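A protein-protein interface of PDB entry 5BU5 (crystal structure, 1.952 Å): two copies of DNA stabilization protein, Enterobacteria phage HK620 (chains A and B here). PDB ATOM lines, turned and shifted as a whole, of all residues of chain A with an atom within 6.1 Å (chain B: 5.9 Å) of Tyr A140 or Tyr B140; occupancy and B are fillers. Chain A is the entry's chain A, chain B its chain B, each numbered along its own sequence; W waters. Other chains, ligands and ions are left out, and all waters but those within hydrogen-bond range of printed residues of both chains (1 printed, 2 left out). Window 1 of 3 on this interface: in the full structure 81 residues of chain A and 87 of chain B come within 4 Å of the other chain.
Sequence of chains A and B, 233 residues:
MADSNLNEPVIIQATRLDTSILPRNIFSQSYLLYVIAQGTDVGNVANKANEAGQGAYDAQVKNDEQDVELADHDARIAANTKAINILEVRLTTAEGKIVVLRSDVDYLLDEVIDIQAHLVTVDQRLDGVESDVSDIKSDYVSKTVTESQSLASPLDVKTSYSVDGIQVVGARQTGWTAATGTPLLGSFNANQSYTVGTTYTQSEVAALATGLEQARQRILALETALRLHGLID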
ATOM      1  N   ASP A 135       5.386  24.295 -12.463  1.00  0.00           N
ATOM      2  CA  ASP A 135       5.702  25.718 -12.546  1.00  0.00           C
ATOM      3  C   ASP A 135       7.004  26.040 -11.821  1.00  0.00           C
ATOM      4  O   ASP A 135       7.838  26.779 -12.334  1.00  0.00           O
ATOM      5  CB  ASP A 135       4.564  26.562 -11.967  1.00  0.00           C
ATOM      6  CG  ASP A 135       3.322  26.542 -12.835  1.00  0.00           C
ATOM      7  OD1 ASP A 135       3.420  26.122 -14.008  1.00  0.00           O
ATOM      8  OD2 ASP A 135       2.250  26.959 -12.349  1.00  0.00           O
ATOM      9  N   ILE A 136       7.170  25.484 -10.625  1.00  0.00           N
ATOM     10  CA  ILE A 136       8.399  25.679  -9.863  1.00  0.00           C
ATOM     11  C   ILE A 136       9.598  25.125 -10.621  1.00  0.00           C
ATOM     12  O   ILE A 136      10.629  25.788 -10.727  1.00  0.00           O
ATOM     13  CB  ILE A 136       8.318  25.015  -8.478  1.00  0.00           C
ATOM     14  CG1 ILE A 136       7.295  25.741  -7.605  1.00  0.00           C
ATOM     15  CG2 ILE A 136       9.677  25.035  -7.800  1.00  0.00           C
ATOM     16  CD1 ILE A 136       6.914  24.986  -6.349  1.00  0.00           C
ATOM     17  N   LYS A 137       9.449  23.916 -11.157  1.00  0.00           N
ATOM     18  CA  LYS A 137      10.521  23.259 -11.900  1.00  0.00           C
ATOM     19  C   LYS A 137      11.066  24.122 -13.034  1.00  0.00           C
ATOM     20  O   LYS A 137      12.271  24.156 -13.273  1.00  0.00           O
ATOM     21  CB  LYS A 137      10.042  21.923 -12.472  1.00  0.00           C
ATOM     22  CG  LYS A 137      10.376  20.717 -11.615  1.00  0.00           C
ATOM     23  CD  LYS A 137      10.156  19.430 -12.394  1.00  0.00           C
ATOM     24  CE  LYS A 137      10.168  18.216 -11.485  1.00  0.00           C
ATOM     25  NZ  LYS A 137      10.121  16.953 -12.274  1.00  0.00           N
ATOM     26  N   SER A 138      10.180  24.801 -13.747  1.00  0.00           N
ATOM     27  CA  SER A 138      10.619  25.625 -14.861  1.00  0.00           C
ATOM     28  C   SER A 138      11.092  27.014 -14.420  1.00  0.00           C
ATOM     29  O   SER A 138      11.823  27.684 -15.151  1.00  0.00           O
ATOM     30  CB  SER A 138       9.493  25.758 -15.888  1.00  0.00           C
ATOM     31  OG  SER A 138       8.362  26.391 -15.322  1.00  0.00           O
ATOM     32  N   ASP A 139      10.640  27.459 -13.250  1.00  0.00           N
ATOM     33  CA  ASP A 139      10.930  28.816 -12.785  1.00  0.00           C
ATOM     34  C   ASP A 139      12.109  28.988 -11.809  1.00  0.00           C
ATOM     35  O   ASP A 139      12.571  30.110 -11.596  1.00  0.00           O
ATOM     36  CB  ASP A 139       9.667  29.389 -12.133  1.00  0.00           C
ATOM     37  CG  ASP A 139       9.728  30.891 -11.954  1.00  0.00           C
ATOM     38  OD1 ASP A 139      10.118  31.591 -12.909  1.00  0.00           O
ATOM     39  OD2 ASP A 139       9.386  31.371 -10.855  1.00  0.00           O
ATOM     40  N   TYR A 140      12.625  27.897 -11.247  1.00  0.00           N
ATOM     41  CA  TYR A 140      13.537  28.020 -10.105  1.00  0.00           C
ATOM     42  C   TYR A 140      15.010  27.997 -10.499  1.00  0.00           C
ATOM     43  O   TYR A 140      15.400  27.353 -11.471  1.00  0.00           O
ATOM     44  CB  TYR A 140      13.254  26.924  -9.069  1.00  0.00           C
ATOM     45  CG  TYR A 140      13.959  25.602  -9.291  1.00  0.00           C
ATOM     46  CD1 TYR A 140      13.416  24.635 -10.126  1.00  0.00           C
ATOM     47  CD2 TYR A 140      15.145  25.302  -8.629  1.00  0.00           C
ATOM     48  CE1 TYR A 140      14.046  23.422 -10.322  1.00  0.00           C
ATOM     49  CE2 TYR A 140      15.782  24.089  -8.819  1.00  0.00           C
ATOM     50  CZ  TYR A 140      15.226  23.152  -9.666  1.00  0.00           C
ATOM     51  OH  TYR A 140      15.850  21.941  -9.864  1.00  0.00           O
ATOM     52  N   VAL A 141      15.822  28.735  -9.752  1.00  0.00           N
ATOM     53  CA  VAL A 141      17.264  28.735  -9.972  1.00  0.00           C
ATOM     54  C   VAL A 141      17.894  27.491  -9.355  1.00  0.00           C
ATOM     55  O   VAL A 141      17.805  27.266  -8.147  1.00  0.00           O
ATOM     56  CB  VAL A 141      17.921  29.990  -9.383  1.00  0.00           C
ATOM     57  CG1 VAL A 141      19.426  29.946  -9.594  1.00  0.00           C
ATOM     58  CG2 VAL A 141      17.315  31.238 -10.006  1.00  0.00           C
ATOM     59  N   SER A 142      18.542  26.695 -10.199  1.00  0.00           N
ATOM     60  CA  SER A 142      19.095  25.407  -9.795  1.00  0.00           C
ATOM     61  C   SER A 142      20.569  25.514  -9.427  1.00  0.00           C
ATOM     62  O   SER A 142      21.315  26.282 -10.031  1.00  0.00           O
ATOM     63  CB  SER A 142      18.909  24.381 -10.913  1.00  0.00           C
ATOM     64  OG  SER A 142      19.793  23.287 -10.750  1.00  0.00           O
ATOM     65  N   LYS A 143      20.984  24.749  -8.423  1.00  0.00           N
ATOM     66  CA  LYS A 143      22.379  24.749  -8.015  1.00  0.00           C
ATOM     67  C   LYS A 143      23.246  23.837  -8.890  1.00  0.00           C
ATOM     68  O   LYS A 143      24.461  24.014  -8.958  1.00  0.00           O
ATOM     69  CB  LYS A 143      22.488  24.323  -6.548  1.00  0.00           C
ATOM     70  CG  LYS A 143      21.877  25.321  -5.567  1.00  0.00           C
ATOM     71  CD  LYS A 143      22.143  24.931  -4.118  1.00  0.00           C
ATOM     72  CE  LYS A 143      21.409  23.650  -3.752  1.00  0.00           C
ATOM     73  NZ  LYS A 143      21.387  23.396  -2.286  1.00  0.00           N
ATOM     74  N   THR A 144      22.628  22.858  -9.544  1.00  0.00           N
ATOM     75  CA  THR A 144      23.376  21.911 -10.374  1.00  0.00           C
ATOM     76  C   THR A 144      23.337  22.118 -11.897  1.00  0.00           C
ATOM     77  O   THR A 144      24.073  21.455 -12.626  1.00  0.00           O
ATOM     78  CB  THR A 144      22.896  20.483 -10.097  1.00  0.00           C
ATOM     79  OG1 THR A 144      21.482  20.411 -10.307  1.00  0.00           O
ATOM     80  CG2 THR A 144      23.209  20.092  -8.659  1.00  0.00           C
ATOM     81  N   GLN A 149      21.862  30.862 -16.065  1.00  0.00           N
ATOM     82  CA  GLN A 149      20.509  31.105 -15.585  1.00  0.00           C
ATOM     83  C   GLN A 149      20.281  32.602 -15.436  1.00  0.00           C
ATOM     84  O   GLN A 149      21.159  33.332 -14.973  1.00  0.00           O
ATOM     85  CB  GLN A 149      20.289  30.389 -14.254  1.00  0.00           C
ATOM     86  CG  GLN A 149      20.386  28.872 -14.356  1.00  0.00           C
ATOM     87  CD  GLN A 149      20.318  28.191 -13.003  1.00  0.00           C
ATOM     88  OE1 GLN A 149      19.245  27.802 -12.540  1.00  0.00           O
ATOM     89  NE2 GLN A 149      21.470  28.042 -12.360  1.00  0.00           N
ATOM     90  N   ASP B 135       5.959  25.715   1.155  1.00  0.00           N
ATOM     91  CA  ASP B 135       7.202  26.171   1.770  1.00  0.00           C
ATOM     92  C   ASP B 135       8.244  26.498   0.710  1.00  0.00           C
ATOM     93  O   ASP B 135       8.935  27.513   0.802  1.00  0.00           O
ATOM     94  CB  ASP B 135       7.754  25.123   2.741  1.00  0.00           C
ATOM     95  CG  ASP B 135       6.917  24.995   3.998  1.00  0.00           C
ATOM     96  OD1 ASP B 135       6.092  25.898   4.257  1.00  0.00           O
ATOM     97  OD2 ASP B 135       7.087  23.997   4.732  1.00  0.00           O
ATOM     98  N   ILE B 136       8.363  25.633  -0.290  1.00  0.00           N
ATOM     99  CA  ILE B 136       9.285  25.878  -1.392  1.00  0.00           C
ATOM    100  C   ILE B 136       8.890  27.150  -2.131  1.00  0.00           C
ATOM    101  O   ILE B 136       9.745  27.978  -2.449  1.00  0.00           O
ATOM    102  CB  ILE B 136       9.328  24.706  -2.384  1.00  0.00           C
ATOM    103  CG1 ILE B 136       9.936  23.472  -1.718  1.00  0.00           C
ATOM    104  CG2 ILE B 136      10.138  25.077  -3.612  1.00  0.00           C
ATOM    105  CD1 ILE B 136       9.737  22.200  -2.506  1.00  0.00           C
ATOM    106  N   LYS B 137       7.593  27.300  -2.388  1.00  0.00           N
ATOM    107  CA  LYS B 137       7.061  28.451  -3.118  1.00  0.00           C
ATOM    108  C   LYS B 137       7.507  29.783  -2.529  1.00  0.00           C
ATOM    109  O   LYS B 137       7.824  30.715  -3.264  1.00  0.00           O
ATOM    110  CB  LYS B 137       5.534  28.402  -3.140  1.00  0.00           C
ATOM    111  CG  LYS B 137       4.928  27.755  -4.369  1.00  0.00           C
ATOM    112  CD  LYS B 137       3.428  28.012  -4.404  1.00  0.00           C
ATOM    113  CE  LYS B 137       2.725  27.103  -5.393  1.00  0.00           C
ATOM    114  NZ  LYS B 137       1.284  27.454  -5.526  1.00  0.00           N
ATOM    115  N   SER B 138       7.519  29.877  -1.205  1.00  0.00           N
ATOM    116  CA  SER B 138       7.912  31.121  -0.557  1.00  0.00           C
ATOM    117  C   SER B 138       9.429  31.271  -0.422  1.00  0.00           C
ATOM    118  O   SER B 138       9.929  32.383  -0.264  1.00  0.00           O
ATOM    119  CB  SER B 138       7.261  31.223   0.823  1.00  0.00           C
ATOM    120  OG  SER B 138       7.689  30.170   1.666  1.00  0.00           O
ATOM    121  N   ASP B 139      10.152  30.156  -0.458  1.00  0.00           N
ATOM    122  CA  ASP B 139      11.594  30.183  -0.215  1.00  0.00           C
ATOM    123  C   ASP B 139      12.507  30.218  -1.457  1.00  0.00           C
ATOM    124  O   ASP B 139      13.706  30.465  -1.327  1.00  0.00           O
ATOM    125  CB  ASP B 139      11.973  28.980   0.655  1.00  0.00           C
ATOM    126  CG  ASP B 139      13.349  29.122   1.282  1.00  0.00           C
ATOM    127  OD1 ASP B 139      13.652  30.218   1.803  1.00  0.00           O
ATOM    128  OD2 ASP B 139      14.119  28.137   1.274  1.00  0.00           O
ATOM    129  N   TYR B 140      11.967  29.991  -2.653  1.00  0.00           N
ATOM    130  CA  TYR B 140      12.845  29.757  -3.806  1.00  0.00           C
ATOM    131  C   TYR B 140      13.091  31.014  -4.635  1.00  0.00           C
ATOM    132  O   TYR B 140      12.233  31.891  -4.728  1.00  0.00           O
ATOM    133  CB  TYR B 140      12.296  28.638  -4.703  1.00  0.00           C
ATOM    134  CG  TYR B 140      11.306  29.062  -5.768  1.00  0.00           C
ATOM    135  CD1 TYR B 140       9.949  29.161  -5.486  1.00  0.00           C
ATOM    136  CD2 TYR B 140      11.727  29.335  -7.065  1.00  0.00           C
ATOM    137  CE1 TYR B 140       9.043  29.538  -6.464  1.00  0.00           C
ATOM    138  CE2 TYR B 140      10.830  29.714  -8.047  1.00  0.00           C
ATOM    139  CZ  TYR B 140       9.490  29.812  -7.743  1.00  0.00           C
ATOM    140  OH  TYR B 140       8.594  30.184  -8.719  1.00  0.00           O
ATOM    141  N   VAL B 141      14.290  31.104  -5.206  1.00  0.00           N
ATOM    142  CA  VAL B 141      14.642  32.207  -6.094  1.00  0.00           C
ATOM    143  C   VAL B 141      14.044  31.975  -7.480  1.00  0.00           C
ATOM    144  O   VAL B 141      14.343  30.976  -8.136  1.00  0.00           O
ATOM    145  CB  VAL B 141      16.171  32.371  -6.215  1.00  0.00           C
ATOM    146  CG1 VAL B 141      16.507  33.517  -7.154  1.00  0.00           C
ATOM    147  CG2 VAL B 141      16.800  32.599  -4.843  1.00  0.00           C
ATOM    148  N   SER B 142      13.208  32.907  -7.925  1.00  0.00           N
ATOM    149  CA  SER B 142      12.475  32.756  -9.181  1.00  0.00           C
ATOM    150  C   SER B 142      13.184  33.424 -10.348  1.00  0.00           C
ATOM    151  O   SER B 142      13.775  34.492 -10.195  1.00  0.00           O
ATOM    152  CB  SER B 142      11.068  33.337  -9.045  1.00  0.00           C
ATOM    153  OG  SER B 142      10.510  33.620 -10.321  1.00  0.00           O
ATOM    154  N   LYS B 143      13.124  32.795 -11.517  1.00  0.00           N
ATOM    155  CA  LYS B 143      13.728  33.378 -12.711  1.00  0.00           C
ATOM    156  C   LYS B 143      12.835  34.406 -13.396  1.00  0.00           C
ATOM    157  O   LYS B 143      13.329  35.232 -14.165  1.00  0.00           O
ATOM    158  CB  LYS B 143      14.109  32.278 -13.709  1.00  0.00           C
ATOM    159  CG  LYS B 143      15.248  31.389 -13.226  1.00  0.00           C
ATOM    160  CD  LYS B 143      15.721  30.419 -14.300  1.00  0.00           C
ATOM    161  CE  LYS B 143      14.662  29.378 -14.613  1.00  0.00           C
ATOM    162  NZ  LYS B 143      15.231  28.259 -15.416  1.00  0.00           N
ATOM    163  N   THR B 144      11.526  34.339 -13.159  1.00  0.00           N
ATOM    164  CA  THR B 144      10.610  35.285 -13.796  1.00  0.00           C
ATOM    165  C   THR B 144      10.068  36.452 -12.954  1.00  0.00           C
ATOM    166  O   THR B 144       9.431  37.345 -13.507  1.00  0.00           O
ATOM    167  CB  THR B 144       9.392  34.537 -14.368  1.00  0.00           C
ATOM    168  OG1 THR B 144       8.763  33.783 -13.327  1.00  0.00           O
ATOM    169  CG2 THR B 144       9.826  33.595 -15.481  1.00  0.00           C
ATOM    170  N   GLN B 149      15.159  40.207  -5.419  1.00  0.00           N
ATOM    171  CA  GLN B 149      15.188  39.057  -4.531  1.00  0.00           C
ATOM    172  C   GLN B 149      16.463  39.086  -3.706  1.00  0.00           C
ATOM    173  O   GLN B 149      17.531  39.420  -4.219  1.00  0.00           O
ATOM    174  CB  GLN B 149      15.094  37.757  -5.327  1.00  0.00           C
ATOM    175  CG  GLN B 149      13.796  37.593  -6.090  1.00  0.00           C
ATOM    176  CD  GLN B 149      13.795  36.357  -6.961  1.00  0.00           C
ATOM    177  OE1 GLN B 149      13.346  35.292  -6.546  1.00  0.00           O
ATOM    178  NE2 GLN B 149      14.299  36.496  -8.185  1.00  0.00           N
HETATM  179  O   HOH W   1      15.504  28.474  -6.365  1.00  0.00           O
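The backbone carbonyl oxygen (O) of Ser A138 lies close to the side-chain amino group (NZ) of Lys B143, 3.5 Å away. The side-chain carboxylate (OD2) of Asp A139 is in hydrogen-bond range of the side-chain hydroxyl (OH) of Tyr B140. OG of Ser B142 is in hydrogen-bond range of OD2 of Asp A139 (2.6 Å). O of Asp A139 is in hydrogen-bond range of N of Lys B143 (2.7 Å). OD1 of Asp A139 lies within hydrogen-bond range of OG1 of Thr B144 (2.6 Å). N of Val A141 is in hydrogen-bond range of O of Val B141, at 3.1 Å.
The side-chain hydroxyl (OG) of Ser A138 sits at hydrogen-bond distance from the backbone carbonyl oxygen (O) of Asp A135, at 3.1 Å. The side-chain hydroxyl (OG) of Ser B142 sits at hydrogen-bond distance from the backbone NH (N) of Thr B144 (3.1 Å). The backbone NH (N) of Ser B142 sits at hydrogen-bond distance from the side-chain amide oxygen (OE1) of Gln B149.
Among the printed residues, merely in contact across the chains: Ile A136 with Lys B137 (3.9 Å), Asp A139 with Val B141 (3.98 Å), Tyr A140 with Tyr B140 (3.5 Å), Tyr A140 with Val B141 (3.6 Å), Tyr A140 with Lys B143 (3.8 Å) and Val A141 with Lys B143 (3.8 Å).
Tyr A140 touches just these residues of chain B: Tyr B140, Val B141 and Lys B143. Of the printed residues of chain A, Thr B144 touches Asp A139. Of the printed residues of chain B, Asp A139 touches Tyr B140, Val B141, Ser B142, Lys B143 and Thr B144. Of the printed residues of chain A, Lys B137 touches Ile A136. Of the printed residues of chain A, Val B141 touches Asp A139 (3.98 Å), Tyr A140 (3.6 Å) and Val A141 (3.1 Å). The nearest residue of chain B that does not touch Tyr A140 is Ser B142 (4.9 Å).
Hydrophobic or aromatic side chains of chain B that line the printed part of chain A: Tyr B140 and Val B141. Of the 11 printed residues of chain A, 5 touch a printed residue of chain B. Printed residues of chain A that touch a printed residue of chain B: Ile A136, Ser A138, Asp A139, Tyr A140 and Val A141. Hydrophobic or aromatic side chains of chain A within 4 Å of the printed part of chain B: Ile A136, Tyr A140 and Val A141. Along chain A the printed residues that touch a printed residue of chain B span positions 136 to 141. Among the printed residues, no Asp or Glu carboxylate lies within 4 Å of a Lys or Arg side-chain nitrogen of the other chain.
Ile A136 touches Lys B137, but with the chains exchanged Lys A137 does not touch Ile B136 (7.7 Å). Asp A139 touches Val B141, but with the chains exchanged Val A141 does not touch Asp B139 (8.6 Å). Asp A139 touches Ser B142, but with the chains exchanged Ser A142 does not touch Asp B139 (10.8 Å). Asp A139 touches Lys B143, but with the chains exchanged Lys A143 does not touch Asp B139 (9.4 Å). 11 positions are printed for both chains.
Water W1 bridges N of Val B141 (3.1 Å) and O of Val A141 (3.2 Å).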
